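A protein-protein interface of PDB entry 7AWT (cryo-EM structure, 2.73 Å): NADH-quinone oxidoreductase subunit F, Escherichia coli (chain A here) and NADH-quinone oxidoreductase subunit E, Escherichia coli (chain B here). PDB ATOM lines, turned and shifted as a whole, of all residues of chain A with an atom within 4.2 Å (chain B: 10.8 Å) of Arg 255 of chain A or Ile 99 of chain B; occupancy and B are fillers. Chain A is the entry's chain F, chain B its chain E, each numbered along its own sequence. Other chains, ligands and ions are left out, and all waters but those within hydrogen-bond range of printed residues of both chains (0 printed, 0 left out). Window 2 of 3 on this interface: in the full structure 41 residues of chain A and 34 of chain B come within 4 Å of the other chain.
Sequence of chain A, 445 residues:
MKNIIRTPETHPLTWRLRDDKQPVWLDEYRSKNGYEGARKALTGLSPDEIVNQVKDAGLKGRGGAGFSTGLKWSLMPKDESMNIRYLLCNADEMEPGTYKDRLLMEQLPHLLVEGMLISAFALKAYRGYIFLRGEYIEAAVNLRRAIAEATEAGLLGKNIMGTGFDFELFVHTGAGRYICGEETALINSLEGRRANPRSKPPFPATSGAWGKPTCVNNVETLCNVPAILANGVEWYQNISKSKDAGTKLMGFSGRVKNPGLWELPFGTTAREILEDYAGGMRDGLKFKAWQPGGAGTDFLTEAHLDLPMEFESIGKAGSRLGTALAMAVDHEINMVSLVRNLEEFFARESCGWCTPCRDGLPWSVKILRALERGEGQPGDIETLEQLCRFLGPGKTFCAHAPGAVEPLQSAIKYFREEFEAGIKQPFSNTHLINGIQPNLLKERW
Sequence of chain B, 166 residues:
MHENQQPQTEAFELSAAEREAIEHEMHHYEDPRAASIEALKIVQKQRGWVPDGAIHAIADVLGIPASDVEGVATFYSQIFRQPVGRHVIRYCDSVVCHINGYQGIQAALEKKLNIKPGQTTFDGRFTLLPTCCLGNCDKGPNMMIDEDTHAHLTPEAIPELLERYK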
ATOM      1  N   GLY A 254      13.270  -6.141 -16.288  1.00  0.00           N
ATOM      2  CA  GLY A 254      13.586  -6.367 -14.894  1.00  0.00           C
ATOM      3  C   GLY A 254      14.865  -7.164 -14.720  1.00  0.00           C
ATOM      4  O   GLY A 254      15.677  -7.310 -15.636  1.00  0.00           O
ATOM      5  N   ARG A 255      15.038  -7.689 -13.512  1.00  0.00           N
ATOM      6  CA  ARG A 255      16.256  -8.412 -13.155  1.00  0.00           C
ATOM      7  C   ARG A 255      16.135  -9.903 -13.445  1.00  0.00           C
ATOM      8  O   ARG A 255      16.394 -10.749 -12.593  1.00  0.00           O
ATOM      9  CB  ARG A 255      16.593  -8.159 -11.693  1.00  0.00           C
ATOM     10  CG  ARG A 255      16.849  -6.701 -11.381  1.00  0.00           C
ATOM     11  CD  ARG A 255      17.834  -6.529 -10.248  1.00  0.00           C
ATOM     12  NE  ARG A 255      17.174  -6.523  -8.948  1.00  0.00           N
ATOM     13  CZ  ARG A 255      17.748  -6.100  -7.829  1.00  0.00           C
ATOM     14  NH1 ARG A 255      17.080  -6.129  -6.686  1.00  0.00           N
ATOM     15  NH2 ARG A 255      18.992  -5.646  -7.853  1.00  0.00           N
ATOM     16  N   VAL A 256      15.737 -10.230 -14.671  1.00  0.00           N
ATOM     17  CA  VAL A 256      15.672 -11.612 -15.132  1.00  0.00           C
ATOM     18  C   VAL A 256      17.028 -12.008 -15.699  1.00  0.00           C
ATOM     19  O   VAL A 256      17.886 -11.152 -15.937  1.00  0.00           O
ATOM     20  CB  VAL A 256      14.554 -11.800 -16.170  1.00  0.00           C
ATOM     21  CG1 VAL A 256      13.206 -11.624 -15.516  1.00  0.00           C
ATOM     22  CG2 VAL A 256      14.717 -10.814 -17.296  1.00  0.00           C
ATOM     23  N   MET A 281      14.384 -15.306 -12.688  1.00  0.00           N
ATOM     24  CA  MET A 281      15.032 -14.406 -11.769  1.00  0.00           C
ATOM     25  C   MET A 281      16.466 -14.844 -11.688  1.00  0.00           C
ATOM     26  O   MET A 281      16.765 -16.016 -11.816  1.00  0.00           O
ATOM     27  CB  MET A 281      14.366 -14.497 -10.418  1.00  0.00           C
ATOM     28  CG  MET A 281      12.912 -14.123 -10.482  1.00  0.00           C
ATOM     29  SD  MET A 281      12.754 -12.558 -11.321  1.00  0.00           S
ATOM     30  CE  MET A 281      13.506 -11.454 -10.149  1.00  0.00           C
ATOM     31  N   ARG A 282      17.363 -13.913 -11.441  1.00  0.00           N
ATOM     32  CA  ARG A 282      18.741 -14.293 -11.505  1.00  0.00           C
ATOM     33  C   ARG A 282      19.570 -14.450 -10.277  1.00  0.00           C
ATOM     34  O   ARG A 282      19.825 -13.509  -9.571  1.00  0.00           O
ATOM     35  CB  ARG A 282      19.464 -13.276 -12.362  1.00  0.00           C
ATOM     36  CG  ARG A 282      19.364 -11.869 -11.834  1.00  0.00           C
ATOM     37  CD  ARG A 282      20.195 -10.946 -12.699  1.00  0.00           C
ATOM     38  NE  ARG A 282      20.164  -9.586 -12.195  1.00  0.00           N
ATOM     39  CZ  ARG A 282      20.756  -8.565 -12.791  1.00  0.00           C
ATOM     40  NH1 ARG A 282      20.666  -7.359 -12.265  1.00  0.00           N
ATOM     41  NH2 ARG A 282      21.439  -8.751 -13.906  1.00  0.00           N
ATOM     42  N   LEU A 285      17.649 -13.990  -6.501  1.00  0.00           N
ATOM     43  CA  LEU A 285      16.485 -13.130  -6.412  1.00  0.00           C
ATOM     44  C   LEU A 285      15.223 -13.979  -6.455  1.00  0.00           C
ATOM     45  O   LEU A 285      15.194 -15.048  -7.069  1.00  0.00           O
ATOM     46  CB  LEU A 285      16.476 -12.110  -7.550  1.00  0.00           C
ATOM     47  CG  LEU A 285      17.219 -10.786  -7.346  1.00  0.00           C
ATOM     48  CD1 LEU A 285      18.537 -10.974  -6.623  1.00  0.00           C
ATOM     49  CD2 LEU A 285      17.449 -10.116  -8.683  1.00  0.00           C
ATOM     50  N   MET A 327       7.347  -6.775 -16.838  1.00  0.00           N
ATOM     51  CA  MET A 327       8.438  -6.331 -15.991  1.00  0.00           C
ATOM     52  C   MET A 327       8.393  -7.219 -14.765  1.00  0.00           C
ATOM     53  O   MET A 327       7.362  -7.356 -14.169  1.00  0.00           O
ATOM     54  CB  MET A 327       8.246  -4.886 -15.596  1.00  0.00           C
ATOM     55  CG  MET A 327       9.386  -4.322 -14.788  1.00  0.00           C
ATOM     56  SD  MET A 327       8.769  -3.031 -13.727  1.00  0.00           S
ATOM     57  CE  MET A 327       7.714  -2.215 -14.905  1.00  0.00           C
ATOM     58  N   ALA A 328       9.510  -7.780 -14.350  1.00  0.00           N
ATOM     59  CA  ALA A 328       9.483  -8.637 -13.194  1.00  0.00           C
ATOM     60  C   ALA A 328      10.052  -7.889 -12.031  1.00  0.00           C
ATOM     61  O   ALA A 328      11.168  -7.436 -12.090  1.00  0.00           O
ATOM     62  CB  ALA A 328      10.304  -9.875 -13.455  1.00  0.00           C
ATOM     63  N   ASP A 330      11.472  -8.137  -8.462  1.00  0.00           N
ATOM     64  CA  ASP A 330      11.965  -9.107  -7.504  1.00  0.00           C
ATOM     65  C   ASP A 330      11.759  -8.665  -6.083  1.00  0.00           C
ATOM     66  O   ASP A 330      11.586  -7.502  -5.806  1.00  0.00           O
ATOM     67  CB  ASP A 330      13.436  -9.345  -7.711  1.00  0.00           C
ATOM     68  CG  ASP A 330      14.217  -8.089  -7.627  1.00  0.00           C
ATOM     69  OD1 ASP A 330      13.838  -7.124  -8.308  1.00  0.00           O
ATOM     70  OD2 ASP A 330      15.212  -8.056  -6.883  1.00  0.00           O
ATOM     71  N   GLU A 332      13.506  -7.809  -3.603  1.00  0.00           N
ATOM     72  CA  GLU A 332      14.258  -6.778  -2.930  1.00  0.00           C
ATOM     73  C   GLU A 332      13.802  -5.377  -3.190  1.00  0.00           C
ATOM     74  O   GLU A 332      14.396  -4.466  -2.699  1.00  0.00           O
ATOM     75  CB  GLU A 332      15.719  -6.893  -3.272  1.00  0.00           C
ATOM     76  CG  GLU A 332      16.362  -8.088  -2.627  1.00  0.00           C
ATOM     77  CD  GLU A 332      17.837  -7.886  -2.384  1.00  0.00           C
ATOM     78  OE1 GLU A 332      18.571  -7.683  -3.365  1.00  0.00           O
ATOM     79  OE2 GLU A 332      18.268  -7.938  -1.213  1.00  0.00           O
ATOM     80  N   ILE A 333      12.777  -5.203  -3.993  1.00  0.00           N
ATOM     81  CA  ILE A 333      12.253  -3.908  -4.310  1.00  0.00           C
ATOM     82  C   ILE A 333      11.133  -3.469  -3.410  1.00  0.00           C
ATOM     83  O   ILE A 333      10.084  -3.988  -3.498  1.00  0.00           O
ATOM     84  CB  ILE A 333      11.613  -4.015  -5.668  1.00  0.00           C
ATOM     85  CG1 ILE A 333      12.665  -4.375  -6.667  1.00  0.00           C
ATOM     86  CG2 ILE A 333      10.976  -2.722  -6.049  1.00  0.00           C
ATOM     87  CD1 ILE A 333      14.017  -3.890  -6.263  1.00  0.00           C
ATOM     88  N   LEU A 338       8.872   1.742  -5.329  1.00  0.00           N
ATOM     89  CA  LEU A 338       8.582   1.515  -6.740  1.00  0.00           C
ATOM     90  C   LEU A 338       7.339   2.276  -7.181  1.00  0.00           C
ATOM     91  O   LEU A 338       7.328   2.901  -8.247  1.00  0.00           O
ATOM     92  CB  LEU A 338       8.417   0.020  -6.998  1.00  0.00           C
ATOM     93  CG  LEU A 338       8.283  -0.432  -8.447  1.00  0.00           C
ATOM     94  CD1 LEU A 338       9.548  -0.125  -9.206  1.00  0.00           C
ATOM     95  CD2 LEU A 338       7.981  -1.910  -8.501  1.00  0.00           C
ATOM     96  N   CYS B  92      18.133   7.879 -17.169  1.00  0.00           N
ATOM     97  CA  CYS B  92      16.733   7.459 -17.085  1.00  0.00           C
ATOM     98  C   CYS B  92      16.420   7.016 -15.695  1.00  0.00           C
ATOM     99  O   CYS B  92      17.188   6.284 -15.108  1.00  0.00           O
ATOM    100  CB  CYS B  92      16.441   6.295 -18.027  1.00  0.00           C
ATOM    101  SG  CYS B  92      14.802   5.525 -17.868  1.00  0.00           S
ATOM    102  N   ASP B  93      15.314   7.493 -15.150  1.00  0.00           N
ATOM    103  CA  ASP B  93      14.905   7.100 -13.824  1.00  0.00           C
ATOM    104  C   ASP B  93      13.442   6.707 -13.808  1.00  0.00           C
ATOM    105  O   ASP B  93      12.627   7.385 -13.225  1.00  0.00           O
ATOM    106  CB  ASP B  93      15.104   8.256 -12.877  1.00  0.00           C
ATOM    107  CG  ASP B  93      14.353   9.455 -13.297  1.00  0.00           C
ATOM    108  OD1 ASP B  93      13.892   9.448 -14.441  1.00  0.00           O
ATOM    109  OD2 ASP B  93      14.207  10.396 -12.499  1.00  0.00           O
ATOM    110  N   SER B  94      13.129   5.584 -14.426  1.00  0.00           N
ATOM    111  CA  SER B  94      11.796   5.022 -14.521  1.00  0.00           C
ATOM    112  C   SER B  94      11.739   3.652 -13.918  1.00  0.00           C
ATOM    113  O   SER B  94      12.733   3.183 -13.440  1.00  0.00           O
ATOM    114  CB  SER B  94      11.183   5.092 -15.879  1.00  0.00           C
ATOM    115  OG  SER B  94      10.989   6.434 -16.219  1.00  0.00           O
ATOM    116  N   VAL B  95      10.625   3.008 -14.014  1.00  0.00           N
ATOM    117  CA  VAL B  95      10.516   1.823 -13.293  1.00  0.00           C
ATOM    118  C   VAL B  95      11.483   0.751 -13.671  1.00  0.00           C
ATOM    119  O   VAL B  95      12.116   0.251 -12.816  1.00  0.00           O
ATOM    120  CB  VAL B  95       9.079   1.430 -13.330  1.00  0.00           C
ATOM    121  CG1 VAL B  95       8.698   1.026 -14.718  1.00  0.00           C
ATOM    122  CG2 VAL B  95       8.788   0.420 -12.273  1.00  0.00           C
ATOM    123  N   VAL B  96      11.705   0.442 -14.925  1.00  0.00           N
ATOM    124  CA  VAL B  96      12.665  -0.584 -15.247  1.00  0.00           C
ATOM    125  C   VAL B  96      14.062  -0.262 -14.821  1.00  0.00           C
ATOM    126  O   VAL B  96      14.814  -1.149 -14.518  1.00  0.00           O
ATOM    127  CB  VAL B  96      12.676  -1.022 -16.676  1.00  0.00           C
ATOM    128  CG1 VAL B  96      13.474  -2.292 -16.742  1.00  0.00           C
ATOM    129  CG2 VAL B  96      11.273  -1.297 -17.118  1.00  0.00           C
ATOM    130  N   CYS B  97      14.455   0.996 -14.893  1.00  0.00           N
ATOM    131  CA  CYS B  97      15.802   1.350 -14.499  1.00  0.00           C
ATOM    132  C   CYS B  97      15.910   1.435 -13.012  1.00  0.00           C
ATOM    133  O   CYS B  97      16.902   0.986 -12.487  1.00  0.00           O
ATOM    134  CB  CYS B  97      16.273   2.598 -15.187  1.00  0.00           C
ATOM    135  SG  CYS B  97      16.717   2.223 -16.870  1.00  0.00           S
ATOM    136  N   HIS B  98      14.908   2.008 -12.341  1.00  0.00           N
ATOM    137  CA  HIS B  98      14.880   2.049 -10.881  1.00  0.00           C
ATOM    138  C   HIS B  98      15.167   0.681 -10.286  1.00  0.00           C
ATOM    139  O   HIS B  98      15.794   0.581  -9.226  1.00  0.00           O
ATOM    140  CB  HIS B  98      13.519   2.560 -10.401  1.00  0.00           C
ATOM    141  CG  HIS B  98      13.288   2.401  -8.931  1.00  0.00           C
ATOM    142  ND1 HIS B  98      13.361   3.459  -8.052  1.00  0.00           N
ATOM    143  CD2 HIS B  98      12.959   1.318  -8.189  1.00  0.00           C
ATOM    144  CE1 HIS B  98      13.106   3.031  -6.830  1.00  0.00           C
ATOM    145  NE2 HIS B  98      12.859   1.736  -6.885  1.00  0.00           N
ATOM    146  N   ILE B  99      14.662  -0.340 -10.943  1.00  0.00           N
ATOM    147  CA  ILE B  99      14.892  -1.709 -10.562  1.00  0.00           C
ATOM    148  C   ILE B  99      16.321  -2.151 -10.779  1.00  0.00           C
ATOM    149  O   ILE B  99      16.892  -2.753  -9.921  1.00  0.00           O
ATOM    150  CB  ILE B  99      13.898  -2.619 -11.251  1.00  0.00           C
ATOM    151  CG1 ILE B  99      12.555  -2.488 -10.578  1.00  0.00           C
ATOM    152  CG2 ILE B  99      14.294  -4.039 -11.087  1.00  0.00           C
ATOM    153  CD1 ILE B  99      11.416  -3.021 -11.387  1.00  0.00           C
ATOM    154  N   ASN B 100      16.908  -1.802 -11.911  1.00  0.00           N
ATOM    155  CA  ASN B 100      18.280  -2.139 -12.260  1.00  0.00           C
ATOM    156  C   ASN B 100      19.306  -1.251 -11.571  1.00  0.00           C
ATOM    157  O   ASN B 100      20.507  -1.517 -11.686  1.00  0.00           O
ATOM    158  CB  ASN B 100      18.468  -2.065 -13.772  1.00  0.00           C
ATOM    159  CG  ASN B 100      17.741  -3.168 -14.499  1.00  0.00           C
ATOM    160  OD1 ASN B 100      18.159  -4.321 -14.470  1.00  0.00           O
ATOM    161  ND2 ASN B 100      16.651  -2.820 -15.161  1.00  0.00           N
ATOM    162  N   GLY B 101      18.872  -0.211 -10.865  1.00  0.00           N
ATOM    163  CA  GLY B 101      19.782   0.578 -10.062  1.00  0.00           C
ATOM    164  C   GLY B 101      20.292   1.846 -10.710  1.00  0.00           C
ATOM    165  O   GLY B 101      21.499   2.097 -10.710  1.00  0.00           O
ATOM    166  N   TYR B 102      19.409   2.681 -11.219  1.00  0.00           N
ATOM    167  CA  TYR B 102      19.844   3.939 -11.785  1.00  0.00           C
ATOM    168  C   TYR B 102      20.237   4.887 -10.675  1.00  0.00           C
ATOM    169  O   TYR B 102      20.775   5.927 -10.955  1.00  0.00           O
ATOM    170  CB  TYR B 102      18.771   4.609 -12.629  1.00  0.00           C
ATOM    171  CG  TYR B 102      17.895   5.500 -11.820  1.00  0.00           C
ATOM    172  CD1 TYR B 102      18.276   6.780 -11.535  1.00  0.00           C
ATOM    173  CD2 TYR B 102      16.692   5.071 -11.354  1.00  0.00           C
ATOM    174  CE1 TYR B 102      17.473   7.613 -10.814  1.00  0.00           C
ATOM    175  CE2 TYR B 102      15.884   5.901 -10.629  1.00  0.00           C
ATOM    176  CZ  TYR B 102      16.281   7.165 -10.371  1.00  0.00           C
ATOM    177  OH  TYR B 102      15.487   8.006  -9.651  1.00  0.00           O
ATOM    178  N   GLN B 103      19.897   4.596  -9.425  1.00  0.00           N
ATOM    179  CA  GLN B 103      20.268   5.487  -8.348  1.00  0.00           C
ATOM    180  C   GLN B 103      21.734   5.528  -8.113  1.00  0.00           C
ATOM    181  O   GLN B 103      22.248   6.540  -7.836  1.00  0.00           O
ATOM    182  CB  GLN B 103      19.566   5.123  -7.098  1.00  0.00           C
ATOM    183  CG  GLN B 103      18.131   5.495  -7.181  1.00  0.00           C
ATOM    184  CD  GLN B 103      17.294   4.387  -6.689  1.00  0.00           C
ATOM    185  OE1 GLN B 103      17.421   3.264  -7.142  1.00  0.00           O
ATOM    186  NE2 GLN B 103      16.445   4.682  -5.734  1.00  0.00           N
ATOM    187  N   GLY B 104      22.406   4.407  -8.129  1.00  0.00           N
ATOM    188  CA  GLY B 104      23.855   4.401  -8.035  1.00  0.00           C
ATOM    189  C   GLY B 104      24.505   5.162  -9.172  1.00  0.00           C
ATOM    190  O   GLY B 104      25.520   5.837  -8.983  1.00  0.00           O
ATOM    191  N   ILE B 105      23.903   5.062 -10.344  1.00  0.00           N
ATOM    192  CA  ILE B 105      24.347   5.758 -11.536  1.00  0.00           C
ATOM    193  C   ILE B 105      24.184   7.241 -11.410  1.00  0.00           C
ATOM    194  O   ILE B 105      24.960   7.930 -11.930  1.00  0.00           O
ATOM    195  CB  ILE B 105      23.717   5.239 -12.813  1.00  0.00           C
ATOM    196  CG1 ILE B 105      24.492   4.062 -13.308  1.00  0.00           C
ATOM    197  CG2 ILE B 105      23.795   6.276 -13.875  1.00  0.00           C
ATOM    198  CD1 ILE B 105      24.460   2.919 -12.338  1.00  0.00           C
ATOM    199  N   CYS B 133      12.082   7.893 -19.998  1.00  0.00           N
ATOM    200  CA  CYS B 133      12.517   6.508 -20.231  1.00  0.00           C
ATOM    201  C   CYS B 133      13.232   6.570 -21.542  1.00  0.00           C
ATOM    202  O   CYS B 133      12.846   7.302 -22.420  1.00  0.00           O
ATOM    203  CB  CYS B 133      11.369   5.494 -20.316  1.00  0.00           C
ATOM    204  SG  CYS B 133      11.796   3.718 -20.488  1.00  0.00           S
ATOM    205  N   CYS B 137      14.905  -0.455 -21.958  1.00  0.00           N
ATOM    206  CA  CYS B 137      14.867  -1.020 -20.618  1.00  0.00           C
ATOM    207  C   CYS B 137      15.539  -2.316 -20.300  1.00  0.00           C
ATOM    208  O   CYS B 137      16.094  -2.465 -19.225  1.00  0.00           O
ATOM    209  CB  CYS B 137      13.430  -1.146 -20.194  1.00  0.00           C
ATOM    210  SG  CYS B 137      12.580   0.362 -20.589  1.00  0.00           S
ATOM    211  N   ASP B 138      15.464  -3.278 -21.188  1.00  0.00           N
ATOM    212  CA  ASP B 138      16.048  -4.552 -20.875  1.00  0.00           C
ATOM    213  C   ASP B 138      17.535  -4.394 -20.708  1.00  0.00           C
ATOM    214  O   ASP B 138      18.194  -5.290 -20.203  1.00  0.00           O
ATOM    215  CB  ASP B 138      15.771  -5.543 -21.983  1.00  0.00           C
ATOM    216  CG  ASP B 138      16.129  -5.001 -23.312  1.00  0.00           C
ATOM    217  OD1 ASP B 138      16.348  -3.789 -23.381  1.00  0.00           O
ATOM    218  OD2 ASP B 138      16.198  -5.765 -24.288  1.00  0.00           O
ATOM    219  N   LYS B 139      18.094  -3.267 -21.127  1.00  0.00           N
ATOM    220  CA  LYS B 139      19.549  -3.186 -21.053  1.00  0.00           C
ATOM    221  C   LYS B 139      19.926  -2.200 -19.950  1.00  0.00           C
ATOM    222  O   LYS B 139      20.208  -1.031 -20.215  1.00  0.00           O
ATOM    223  CB  LYS B 139      20.136  -2.779 -22.394  1.00  0.00           C
ATOM    224  CG  LYS B 139      20.074  -3.872 -23.440  1.00  0.00           C
ATOM    225  CD  LYS B 139      20.156  -3.305 -24.842  1.00  0.00           C
ATOM    226  CE  LYS B 139      19.803  -4.356 -25.877  1.00  0.00           C
ATOM    227  NZ  LYS B 139      19.530  -3.752 -27.206  1.00  0.00           N
ATOM    228  N   GLY B 140      19.924  -2.687 -18.712  1.00  0.00           N
ATOM    229  CA  GLY B 140      20.464  -1.975 -17.577  1.00  0.00           C
ATOM    230  C   GLY B 140      19.921  -0.573 -17.401  1.00  0.00           C
ATOM    231  O   GLY B 140      18.906  -0.192 -17.991  1.00  0.00           O
ATOM    232  N   PRO B 141      20.586   0.220 -16.563  1.00  0.00           N
ATOM    233  CA  PRO B 141      20.245   1.643 -16.459  1.00  0.00           C
ATOM    234  C   PRO B 141      20.842   2.405 -17.632  1.00  0.00           C
ATOM    235  O   PRO B 141      22.024   2.258 -17.947  1.00  0.00           O
ATOM    236  CB  PRO B 141      20.878   2.066 -15.132  1.00  0.00           C
ATOM    237  CG  PRO B 141      21.968   1.091 -14.912  1.00  0.00           C
ATOM    238  CD  PRO B 141      21.549  -0.201 -15.535  1.00  0.00           C
ATOM    239  N   ASN B 142      20.026   3.191 -18.312  1.00  0.00           N
ATOM    240  CA  ASN B 142      20.478   3.905 -19.482  1.00  0.00           C
ATOM    241  C   ASN B 142      20.606   5.366 -19.302  1.00  0.00           C
ATOM    242  O   ASN B 142      20.040   5.939 -18.400  1.00  0.00           O
ATOM    243  CB  ASN B 142      19.473   3.728 -20.582  1.00  0.00           C
ATOM    244  CG  ASN B 142      19.438   2.339 -21.085  1.00  0.00           C
ATOM    245  OD1 ASN B 142      19.797   2.072 -22.217  1.00  0.00           O
ATOM    246  ND2 ASN B 142      19.051   1.434 -20.235  1.00  0.00           N
ATOM    247  N   LEU B 153      24.874   0.602 -17.740  1.00  0.00           N
ATOM    248  CA  LEU B 153      25.702   1.523 -16.980  1.00  0.00           C
ATOM    249  C   LEU B 153      26.095   0.922 -15.641  1.00  0.00           C
ATOM    250  O   LEU B 153      25.280   0.305 -14.952  1.00  0.00           O
ATOM    251  CB  LEU B 153      24.967   2.838 -16.760  1.00  0.00           C
ATOM    252  CG  LEU B 153      24.837   3.747 -17.974  1.00  0.00           C
ATOM    253  CD1 LEU B 153      23.933   4.901 -17.636  1.00  0.00           C
ATOM    254  CD2 LEU B 153      26.197   4.239 -18.404  1.00  0.00           C
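O of Val 96 of chain B is in hydrogen-bond range of ND2 of Asn 100 of chain B (2.6 Å). The guanidinium group (NH1) of Arg 255 of chain A is in salt-bridge range of the side-chain carboxylate (OD2) of Asp 330 of chain A (2.7 Å). The guanidinium group (NH1) of Arg 255 of chain A lies within salt-bridge range of the side-chain carboxylate (OE1) of Glu 332 of chain A (3.96 Å).
Among the printed residues, pairs that only touch across the chains: Leu 338 of chain A with Val 95 of chain B (3.2 Å), Met 327 of chain A with Val 95 of chain B (3.4 Å), Met 327 of chain A with Ile 99 of chain B (3.5 Å), Arg 255 of chain A with Ile 99 of chain B (3.7 Å), Leu 338 of chain A with His 98 of chain B (3.8 Å) and Gly 254 of chain A with Val 96 of chain B (3.9 Å).
Gly 254 of chain A touches just one residue of chain B: Val 96. Arg 255 of chain A touches just one residue of chain B: Ile 99 (3.7 Å). No residue of chain B comes within 4 Å of Met 281 of chain A. Arg 282 of chain A touches none of the printed residues of chain B. Of the printed residues of chain B, Met 327 of chain A touches Val 95 and Ile 99. No residue of chain B comes within 4 Å of Asp 330 of chain A. No residue of chain B comes within 4 Å of Glu 332 of chain A. Of the printed residues of chain A, Val 95 of chain B touches Met 327 and Leu 338. Of the printed residues of chain A, His 98 of chain B touches Leu 338. Of chain A, only Arg 255 (3.7 Å) and Met 327 (3.5 Å) come within 4 Å of Ile 99 of chain B. The nearest residue of chain B that does not touch Arg 255 of chain A is Asn 100 of chain B (4.1 Å). The nearest printed residue of chain A that does not touch His 98 of chain B is Ile 333 of chain A (4.9 Å).
Of the 12 printed residues of chain A, 4 touch a printed residue of chain B. Hydrophobic or aromatic side chains of chain A that line the printed part of chain B: Met 327 and Leu 338.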
